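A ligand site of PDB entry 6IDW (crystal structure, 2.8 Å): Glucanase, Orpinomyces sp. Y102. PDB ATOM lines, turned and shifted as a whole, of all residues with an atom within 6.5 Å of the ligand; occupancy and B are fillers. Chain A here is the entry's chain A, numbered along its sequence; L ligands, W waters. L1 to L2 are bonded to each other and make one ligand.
The backbone carbonyl oxygen of Asp 121 lies within hydrogen-bond range of the side-chain amide nitrogen of Asn 125 (2.8 Å).
ND2 of Asn 202 lies within hydrogen-bond range of NE2 of His 166, at 3.3 Å.
ND1 of His 166 sits at hydrogen-bond distance from N of Gly 168 (3.0 Å).
The backbone NH (N) of Trp 169 sits close to a ring nitrogen (ND1) of His 166, at 3.4 Å.
The side-chain amide nitrogen of Gln 204 sits at hydrogen-bond distance from the side-chain amide oxygen of Asn 202 (2.9 Å).
The side-chain amide oxygen (OD1) of Asn 199 lies close to the backbone carbonyl oxygen (O) of Asn 202, at 3.1 Å.
The side-chain hydroxyl of Thr 128 lies within hydrogen-bond range of the indole nitrogen of Trp 169, at 2.8 Å.
The side-chain carboxylate (OD2) of Asp 121 sits at hydrogen-bond distance from an oxygen (O3) of LG2 L2.
O2 of LIG L1 lies close to NE2 of His 166.
The side-chain amide nitrogen (ND2) of Asn 202 is in hydrogen-bond range of an oxygen (O5) of LG2 L2, at 3.2 Å.
Water W2 lies within hydrogen-bond range of the backbone carbonyl oxygen (O) of Val 200 and an oxygen (O5) of LG2 L2.
Water W5 lies within hydrogen-bond range of an oxygen (O2) of LIG L1 (2.8 Å), the backbone carbonyl oxygen of Ala 244 (2.8 Å) and the side-chain amide nitrogen of Asn 202 (3.1 Å).
Water W3 bridges ND2 of Asn 125 (3.0 Å) and O1 of LG2 L2 (3.1 Å).
Water W4 lies within hydrogen-bond range of OG1 of Thr 128 (2.9 Å), O6 of LIG L1 (3.2 Å) and OD1 of Asn 125 (3.4 Å).
Water W1 lies within hydrogen-bond range of the side-chain carboxylate (OD2) of Asp 121, the backbone carbonyl oxygen (O) of Val 200 and an oxygen (O3) of LG2 L2.
Gly 168 touches the ligand.
Trp 169 touches the ligand.
O of Val 200 touches O5 of LG2 L2, at 3.7 Å.
O of Ser 201 touches C5 of LG2 L2, 3.9 Å away.
Trp 246 touches the ligand.
Hydrophobic or aromatic side chains within 4 Å of the ligand: His 166, Trp 169 and Trp 246.
Eight residues have an atom within 4 Å of the ligand: Asp 121, His 166, Gly 168, Trp 169, Val 200, Ser 201, Asn 202 and Trp 246.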
ATOM      1  N   TYR A  73      -9.275 -29.427 -17.387  1.00  0.00           N
ATOM      2  CA  TYR A  73      -8.905 -28.069 -17.859  1.00  0.00           C
ATOM      3  C   TYR A  73      -8.219 -28.112 -19.231  1.00  0.00           C
ATOM      4  O   TYR A  73      -7.062 -27.712 -19.415  1.00  0.00           O
ATOM      5  CB  TYR A  73      -8.026 -27.395 -16.813  1.00  0.00           C
ATOM      6  CG  TYR A  73      -7.797 -25.926 -17.039  1.00  0.00           C
ATOM      7  CD1 TYR A  73      -8.862 -25.046 -17.147  1.00  0.00           C
ATOM      8  CD2 TYR A  73      -6.495 -25.414 -17.081  1.00  0.00           C
ATOM      9  CE1 TYR A  73      -8.645 -23.696 -17.323  1.00  0.00           C
ATOM     10  CE2 TYR A  73      -6.272 -24.072 -17.261  1.00  0.00           C
ATOM     11  CZ  TYR A  73      -7.356 -23.212 -17.404  1.00  0.00           C
ATOM     12  OH  TYR A  73      -7.141 -21.882 -17.619  1.00  0.00           O
ATOM     13  N   PRO A 120     -12.475 -24.845 -15.144  1.00  0.00           N
ATOM     14  CA  PRO A 120     -12.413 -23.530 -14.539  1.00  0.00           C
ATOM     15  C   PRO A 120     -12.358 -22.360 -15.592  1.00  0.00           C
ATOM     16  O   PRO A 120     -11.735 -22.575 -16.663  1.00  0.00           O
ATOM     17  CB  PRO A 120     -11.134 -23.582 -13.686  1.00  0.00           C
ATOM     18  CG  PRO A 120     -10.939 -25.032 -13.463  1.00  0.00           C
ATOM     19  CD  PRO A 120     -11.429 -25.730 -14.711  1.00  0.00           C
ATOM     20  N   ASP A 121     -12.992 -21.208 -15.313  1.00  0.00           N
ATOM     21  CA  ASP A 121     -12.989 -20.000 -16.142  1.00  0.00           C
ATOM     22  C   ASP A 121     -13.699 -20.118 -17.493  1.00  0.00           C
ATOM     23  O   ASP A 121     -13.494 -19.254 -18.346  1.00  0.00           O
ATOM     24  CB  ASP A 121     -11.587 -19.374 -16.272  1.00  0.00           C
ATOM     25  CG  ASP A 121     -10.876 -19.212 -14.919  1.00  0.00           C
ATOM     26  OD1 ASP A 121     -11.354 -18.459 -14.025  1.00  0.00           O
ATOM     27  OD2 ASP A 121      -9.809 -19.840 -14.748  1.00  0.00           O
ATOM     28  N   ASN A 125     -16.347 -16.676 -18.505  1.00  0.00           N
ATOM     29  CA  ASN A 125     -16.148 -16.042 -19.803  1.00  0.00           C
ATOM     30  C   ASN A 125     -17.416 -16.037 -20.640  1.00  0.00           C
ATOM     31  O   ASN A 125     -17.660 -15.054 -21.312  1.00  0.00           O
ATOM     32  CB  ASN A 125     -14.980 -16.689 -20.570  1.00  0.00           C
ATOM     33  CG  ASN A 125     -13.627 -16.314 -20.012  1.00  0.00           C
ATOM     34  OD1 ASN A 125     -13.430 -15.195 -19.557  1.00  0.00           O
ATOM     35  ND2 ASN A 125     -12.677 -17.242 -20.038  1.00  0.00           N
ATOM     36  N   THR A 128     -19.415 -13.018 -19.208  1.00  0.00           N
ATOM     37  CA  THR A 128     -18.887 -11.649 -19.143  1.00  0.00           C
ATOM     38  C   THR A 128     -18.058 -11.246 -20.346  1.00  0.00           C
ATOM     39  O   THR A 128     -17.998 -10.059 -20.649  1.00  0.00           O
ATOM     40  CB  THR A 128     -18.085 -11.363 -17.840  1.00  0.00           C
ATOM     41  OG1 THR A 128     -16.967 -12.262 -17.726  1.00  0.00           O
ATOM     42  CG2 THR A 128     -18.950 -11.456 -16.593  1.00  0.00           C
ATOM     43  N   ALA A 165     -16.974 -19.608 -11.663  1.00  0.00           N
ATOM     44  CA  ALA A 165     -16.230 -18.406 -11.266  1.00  0.00           C
ATOM     45  C   ALA A 165     -16.078 -18.091  -9.785  1.00  0.00           C
ATOM     46  O   ALA A 165     -15.664 -18.948  -9.005  1.00  0.00           O
ATOM     47  CB  ALA A 165     -16.739 -17.200 -12.070  1.00  0.00           C
ATOM     48  N   HIS A 166     -16.376 -16.848  -9.427  1.00  0.00           N
ATOM     49  CA  HIS A 166     -16.346 -16.406  -8.045  1.00  0.00           C
ATOM     50  C   HIS A 166     -17.268 -15.180  -7.968  1.00  0.00           C
ATOM     51  O   HIS A 166     -17.651 -14.568  -8.997  1.00  0.00           O
ATOM     52  CB  HIS A 166     -14.941 -16.128  -7.473  1.00  0.00           C
ATOM     53  CG  HIS A 166     -14.213 -15.066  -8.217  1.00  0.00           C
ATOM     54  ND1 HIS A 166     -14.348 -13.730  -7.923  1.00  0.00           N
ATOM     55  CD2 HIS A 166     -13.343 -15.137  -9.262  1.00  0.00           C
ATOM     56  CE1 HIS A 166     -13.620 -13.011  -8.769  1.00  0.00           C
ATOM     57  NE2 HIS A 166     -13.005 -13.842  -9.597  1.00  0.00           N
ATOM     58  N   GLY A 168     -16.695 -12.126  -6.915  1.00  0.00           N
ATOM     59  CA  GLY A 168     -16.144 -10.907  -7.480  1.00  0.00           C
ATOM     60  C   GLY A 168     -16.403 -10.772  -8.971  1.00  0.00           C
ATOM     61  O   GLY A 168     -16.381  -9.680  -9.501  1.00  0.00           O
ATOM     62  N   TRP A 169     -16.648 -11.886  -9.640  1.00  0.00           N
ATOM     63  CA  TRP A 169     -16.814 -11.939 -11.088  1.00  0.00           C
ATOM     64  C   TRP A 169     -18.306 -12.015 -11.523  1.00  0.00           C
ATOM     65  O   TRP A 169     -18.741 -11.297 -12.427  1.00  0.00           O
ATOM     66  CB  TRP A 169     -16.070 -13.210 -11.572  1.00  0.00           C
ATOM     67  CG  TRP A 169     -15.826 -13.383 -13.077  1.00  0.00           C
ATOM     68  CD1 TRP A 169     -16.401 -12.693 -14.089  1.00  0.00           C
ATOM     69  CD2 TRP A 169     -14.928 -14.326 -13.700  1.00  0.00           C
ATOM     70  NE1 TRP A 169     -15.919 -13.113 -15.311  1.00  0.00           N
ATOM     71  CE2 TRP A 169     -15.021 -14.125 -15.107  1.00  0.00           C
ATOM     72  CE3 TRP A 169     -14.066 -15.322 -13.222  1.00  0.00           C
ATOM     73  CZ2 TRP A 169     -14.280 -14.875 -16.030  1.00  0.00           C
ATOM     74  CZ3 TRP A 169     -13.316 -16.071 -14.156  1.00  0.00           C
ATOM     75  CH2 TRP A 169     -13.448 -15.845 -15.539  1.00  0.00           C
ATOM     76  N   LEU A 170     -19.086 -12.879 -10.872  1.00  0.00           N
ATOM     77  CA  LEU A 170     -20.421 -13.199 -11.341  1.00  0.00           C
ATOM     78  C   LEU A 170     -21.596 -12.913 -10.378  1.00  0.00           C
ATOM     79  O   LEU A 170     -22.750 -13.087 -10.774  1.00  0.00           O
ATOM     80  CB  LEU A 170     -20.447 -14.660 -11.754  1.00  0.00           C
ATOM     81  CG  LEU A 170     -19.671 -15.036 -13.006  1.00  0.00           C
ATOM     82  CD1 LEU A 170     -19.958 -16.505 -13.297  1.00  0.00           C
ATOM     83  CD2 LEU A 170     -19.987 -14.158 -14.211  1.00  0.00           C
ATOM     84  N   ASN A 199     -14.403 -19.941  -6.831  1.00  0.00           N
ATOM     85  CA  ASN A 199     -13.265 -19.274  -6.250  1.00  0.00           C
ATOM     86  C   ASN A 199     -12.010 -20.021  -6.662  1.00  0.00           C
ATOM     87  O   ASN A 199     -10.923 -19.915  -5.992  1.00  0.00           O
ATOM     88  CB  ASN A 199     -13.352 -19.193  -4.699  1.00  0.00           C
ATOM     89  CG  ASN A 199     -12.400 -18.178  -4.144  1.00  0.00           C
ATOM     90  OD1 ASN A 199     -12.144 -17.167  -4.786  1.00  0.00           O
ATOM     91  ND2 ASN A 199     -11.831 -18.451  -2.996  1.00  0.00           N
ATOM     92  N   VAL A 200     -12.165 -20.804  -7.744  1.00  0.00           N
ATOM     93  CA  VAL A 200     -11.053 -21.621  -8.249  1.00  0.00           C
ATOM     94  C   VAL A 200      -9.961 -20.703  -8.749  1.00  0.00           C
ATOM     95  O   VAL A 200     -10.196 -19.861  -9.675  1.00  0.00           O
ATOM     96  CB  VAL A 200     -11.473 -22.640  -9.310  1.00  0.00           C
ATOM     97  CG1 VAL A 200     -10.259 -23.334  -9.910  1.00  0.00           C
ATOM     98  CG2 VAL A 200     -12.352 -23.695  -8.673  1.00  0.00           C
ATOM     99  N   SER A 201      -8.777 -20.836  -8.106  1.00  0.00           N
ATOM    100  CA  SER A 201      -7.622 -20.020  -8.445  1.00  0.00           C
ATOM    101  C   SER A 201      -7.845 -18.567  -8.129  1.00  0.00           C
ATOM    102  O   SER A 201      -7.163 -17.718  -8.706  1.00  0.00           O
ATOM    103  CB  SER A 201      -7.262 -20.122  -9.935  1.00  0.00           C
ATOM    104  OG  SER A 201      -6.639 -21.348 -10.225  1.00  0.00           O
ATOM    105  N   ASN A 202      -8.737 -18.279  -7.171  1.00  0.00           N
ATOM    106  CA  ASN A 202      -9.021 -16.899  -6.713  1.00  0.00           C
ATOM    107  C   ASN A 202      -8.988 -16.785  -5.172  1.00  0.00           C
ATOM    108  O   ASN A 202      -9.101 -17.780  -4.467  1.00  0.00           O
ATOM    109  CB  ASN A 202     -10.306 -16.311  -7.326  1.00  0.00           C
ATOM    110  CG  ASN A 202     -10.229 -14.791  -7.513  1.00  0.00           C
ATOM    111  OD1 ASN A 202     -10.460 -14.016  -6.587  1.00  0.00           O
ATOM    112  ND2 ASN A 202      -9.859 -14.377  -8.712  1.00  0.00           N
ATOM    113  N   GLN A 204     -11.113 -14.913  -2.958  1.00  0.00           N
ATOM    114  CA  GLN A 204     -12.314 -14.470  -2.234  1.00  0.00           C
ATOM    115  C   GLN A 204     -12.540 -15.161  -0.886  1.00  0.00           C
ATOM    116  O   GLN A 204     -12.318 -16.365  -0.754  1.00  0.00           O
ATOM    117  CB  GLN A 204     -13.574 -14.709  -3.070  1.00  0.00           C
ATOM    118  CG  GLN A 204     -13.527 -14.177  -4.489  1.00  0.00           C
ATOM    119  CD  GLN A 204     -13.298 -12.688  -4.532  1.00  0.00           C
ATOM    120  OE1 GLN A 204     -14.141 -11.885  -4.153  1.00  0.00           O
ATOM    121  NE2 GLN A 204     -12.144 -12.313  -5.005  1.00  0.00           N
ATOM    122  N   ALA A 244      -8.771  -6.707  -7.594  1.00  0.00           N
ATOM    123  CA  ALA A 244      -9.171  -7.762  -8.556  1.00  0.00           C
ATOM    124  C   ALA A 244      -8.017  -8.436  -9.408  1.00  0.00           C
ATOM    125  O   ALA A 244      -8.312  -9.252 -10.313  1.00  0.00           O
ATOM    126  CB  ALA A 244     -10.297  -7.241  -9.433  1.00  0.00           C
ATOM    127  N   THR A 245      -6.747  -8.112  -9.132  1.00  0.00           N
ATOM    128  CA  THR A 245      -5.605  -8.819  -9.738  1.00  0.00           C
ATOM    129  C   THR A 245      -5.742 -10.334  -9.417  1.00  0.00           C
ATOM    130  O   THR A 245      -5.849 -10.734  -8.220  1.00  0.00           O
ATOM    131  CB  THR A 245      -4.286  -8.270  -9.194  1.00  0.00           C
ATOM    132  OG1 THR A 245      -4.144  -6.914  -9.598  1.00  0.00           O
ATOM    133  CG2 THR A 245      -3.088  -9.045  -9.719  1.00  0.00           C
ATOM    134  N   TRP A 246      -5.787 -11.141 -10.482  1.00  0.00           N
ATOM    135  CA  TRP A 246      -5.979 -12.608 -10.362  1.00  0.00           C
ATOM    136  C   TRP A 246      -4.626 -13.345 -10.434  1.00  0.00           C
ATOM    137  O   TRP A 246      -4.475 -14.459  -9.898  1.00  0.00           O
ATOM    138  CB  TRP A 246      -6.985 -13.140 -11.428  1.00  0.00           C
ATOM    139  CG  TRP A 246      -6.519 -12.861 -12.826  1.00  0.00           C
ATOM    140  CD1 TRP A 246      -6.832 -11.770 -13.591  1.00  0.00           C
ATOM    141  CD2 TRP A 246      -5.583 -13.627 -13.597  1.00  0.00           C
ATOM    142  NE1 TRP A 246      -6.163 -11.818 -14.784  1.00  0.00           N
ATOM    143  CE2 TRP A 246      -5.375 -12.938 -14.812  1.00  0.00           C
ATOM    144  CE3 TRP A 246      -4.881 -14.835 -13.369  1.00  0.00           C
ATOM    145  CZ2 TRP A 246      -4.489 -13.406 -15.819  1.00  0.00           C
ATOM    146  CZ3 TRP A 246      -4.014 -15.313 -14.382  1.00  0.00           C
ATOM    147  CH2 TRP A 246      -3.825 -14.591 -15.585  1.00  0.00           C
HETATM  148  C1  LIG L   1     -12.326 -11.554 -11.856  1.00  0.00           C
HETATM  149  C2  LIG L   1     -11.052 -12.177 -12.423  1.00  0.00           C
HETATM  150  C3  LIG L   1     -11.232 -12.502 -13.900  1.00  0.00           C
HETATM  151  C4  LIG L   1     -11.795 -11.308 -14.667  1.00  0.00           C
HETATM  152  C5  LIG L   1     -12.034 -11.664 -16.128  1.00  0.00           C
HETATM  153  C6  LIG L   1     -12.822 -10.418 -12.734  1.00  0.00           C
HETATM  154  O1  LIG L   1     -14.064  -9.910 -12.218  1.00  0.00           O
HETATM  155  O2  LIG L   1     -12.061 -11.051 -10.535  1.00  0.00           O
HETATM  156  O3  LIG L   1     -10.749 -13.376 -11.708  1.00  0.00           O
HETATM  157  O4  LIG L   1      -9.971 -12.875 -14.462  1.00  0.00           O
HETATM  158  O5  LIG L   1     -13.015 -10.896 -14.069  1.00  0.00           O
HETATM  159  O6  LIG L   1     -12.557 -10.519 -16.817  1.00  0.00           O
HETATM  160  C1  LG2 L   2      -8.681 -14.633 -15.481  1.00  0.00           C
HETATM  161  C2  LG2 L   2      -8.413 -16.133 -15.503  1.00  0.00           C
HETATM  162  C3  LG2 L   2      -8.273 -16.679 -14.095  1.00  0.00           C
HETATM  163  C4  LG2 L   2      -9.435 -16.220 -13.217  1.00  0.00           C
HETATM  164  C5  LG2 L   2      -9.261 -16.708 -11.788  1.00  0.00           C
HETATM  165  C6  LG2 L   2      -9.811 -14.290 -14.525  1.00  0.00           C
HETATM  166  O1  LG2 L   2      -9.029 -14.191 -16.799  1.00  0.00           O
HETATM  167  O2  LG2 L   2      -7.202 -16.388 -16.233  1.00  0.00           O
HETATM  168  O3  LG2 L   2      -8.250 -18.106 -14.135  1.00  0.00           O
HETATM  169  O4  LG2 L   2      -9.497 -14.790 -13.228  1.00  0.00           O
HETATM  170  O5  LG2 L   2     -10.451 -16.433 -11.042  1.00  0.00           O
HETATM  171  O   HOH W   1      -9.666 -20.771 -12.372  1.00  0.00           O
HETATM  172  O   HOH W   2     -12.058 -18.301 -10.022  1.00  0.00           O
HETATM  173  O   HOH W   3     -10.138 -16.315 -18.779  1.00  0.00           O
HETATM  174  O   HOH W   4     -14.402 -11.984 -18.977  1.00  0.00           O
HETATM  175  O   HOH W   5      -9.726 -11.346  -9.075  1.00  0.00           O
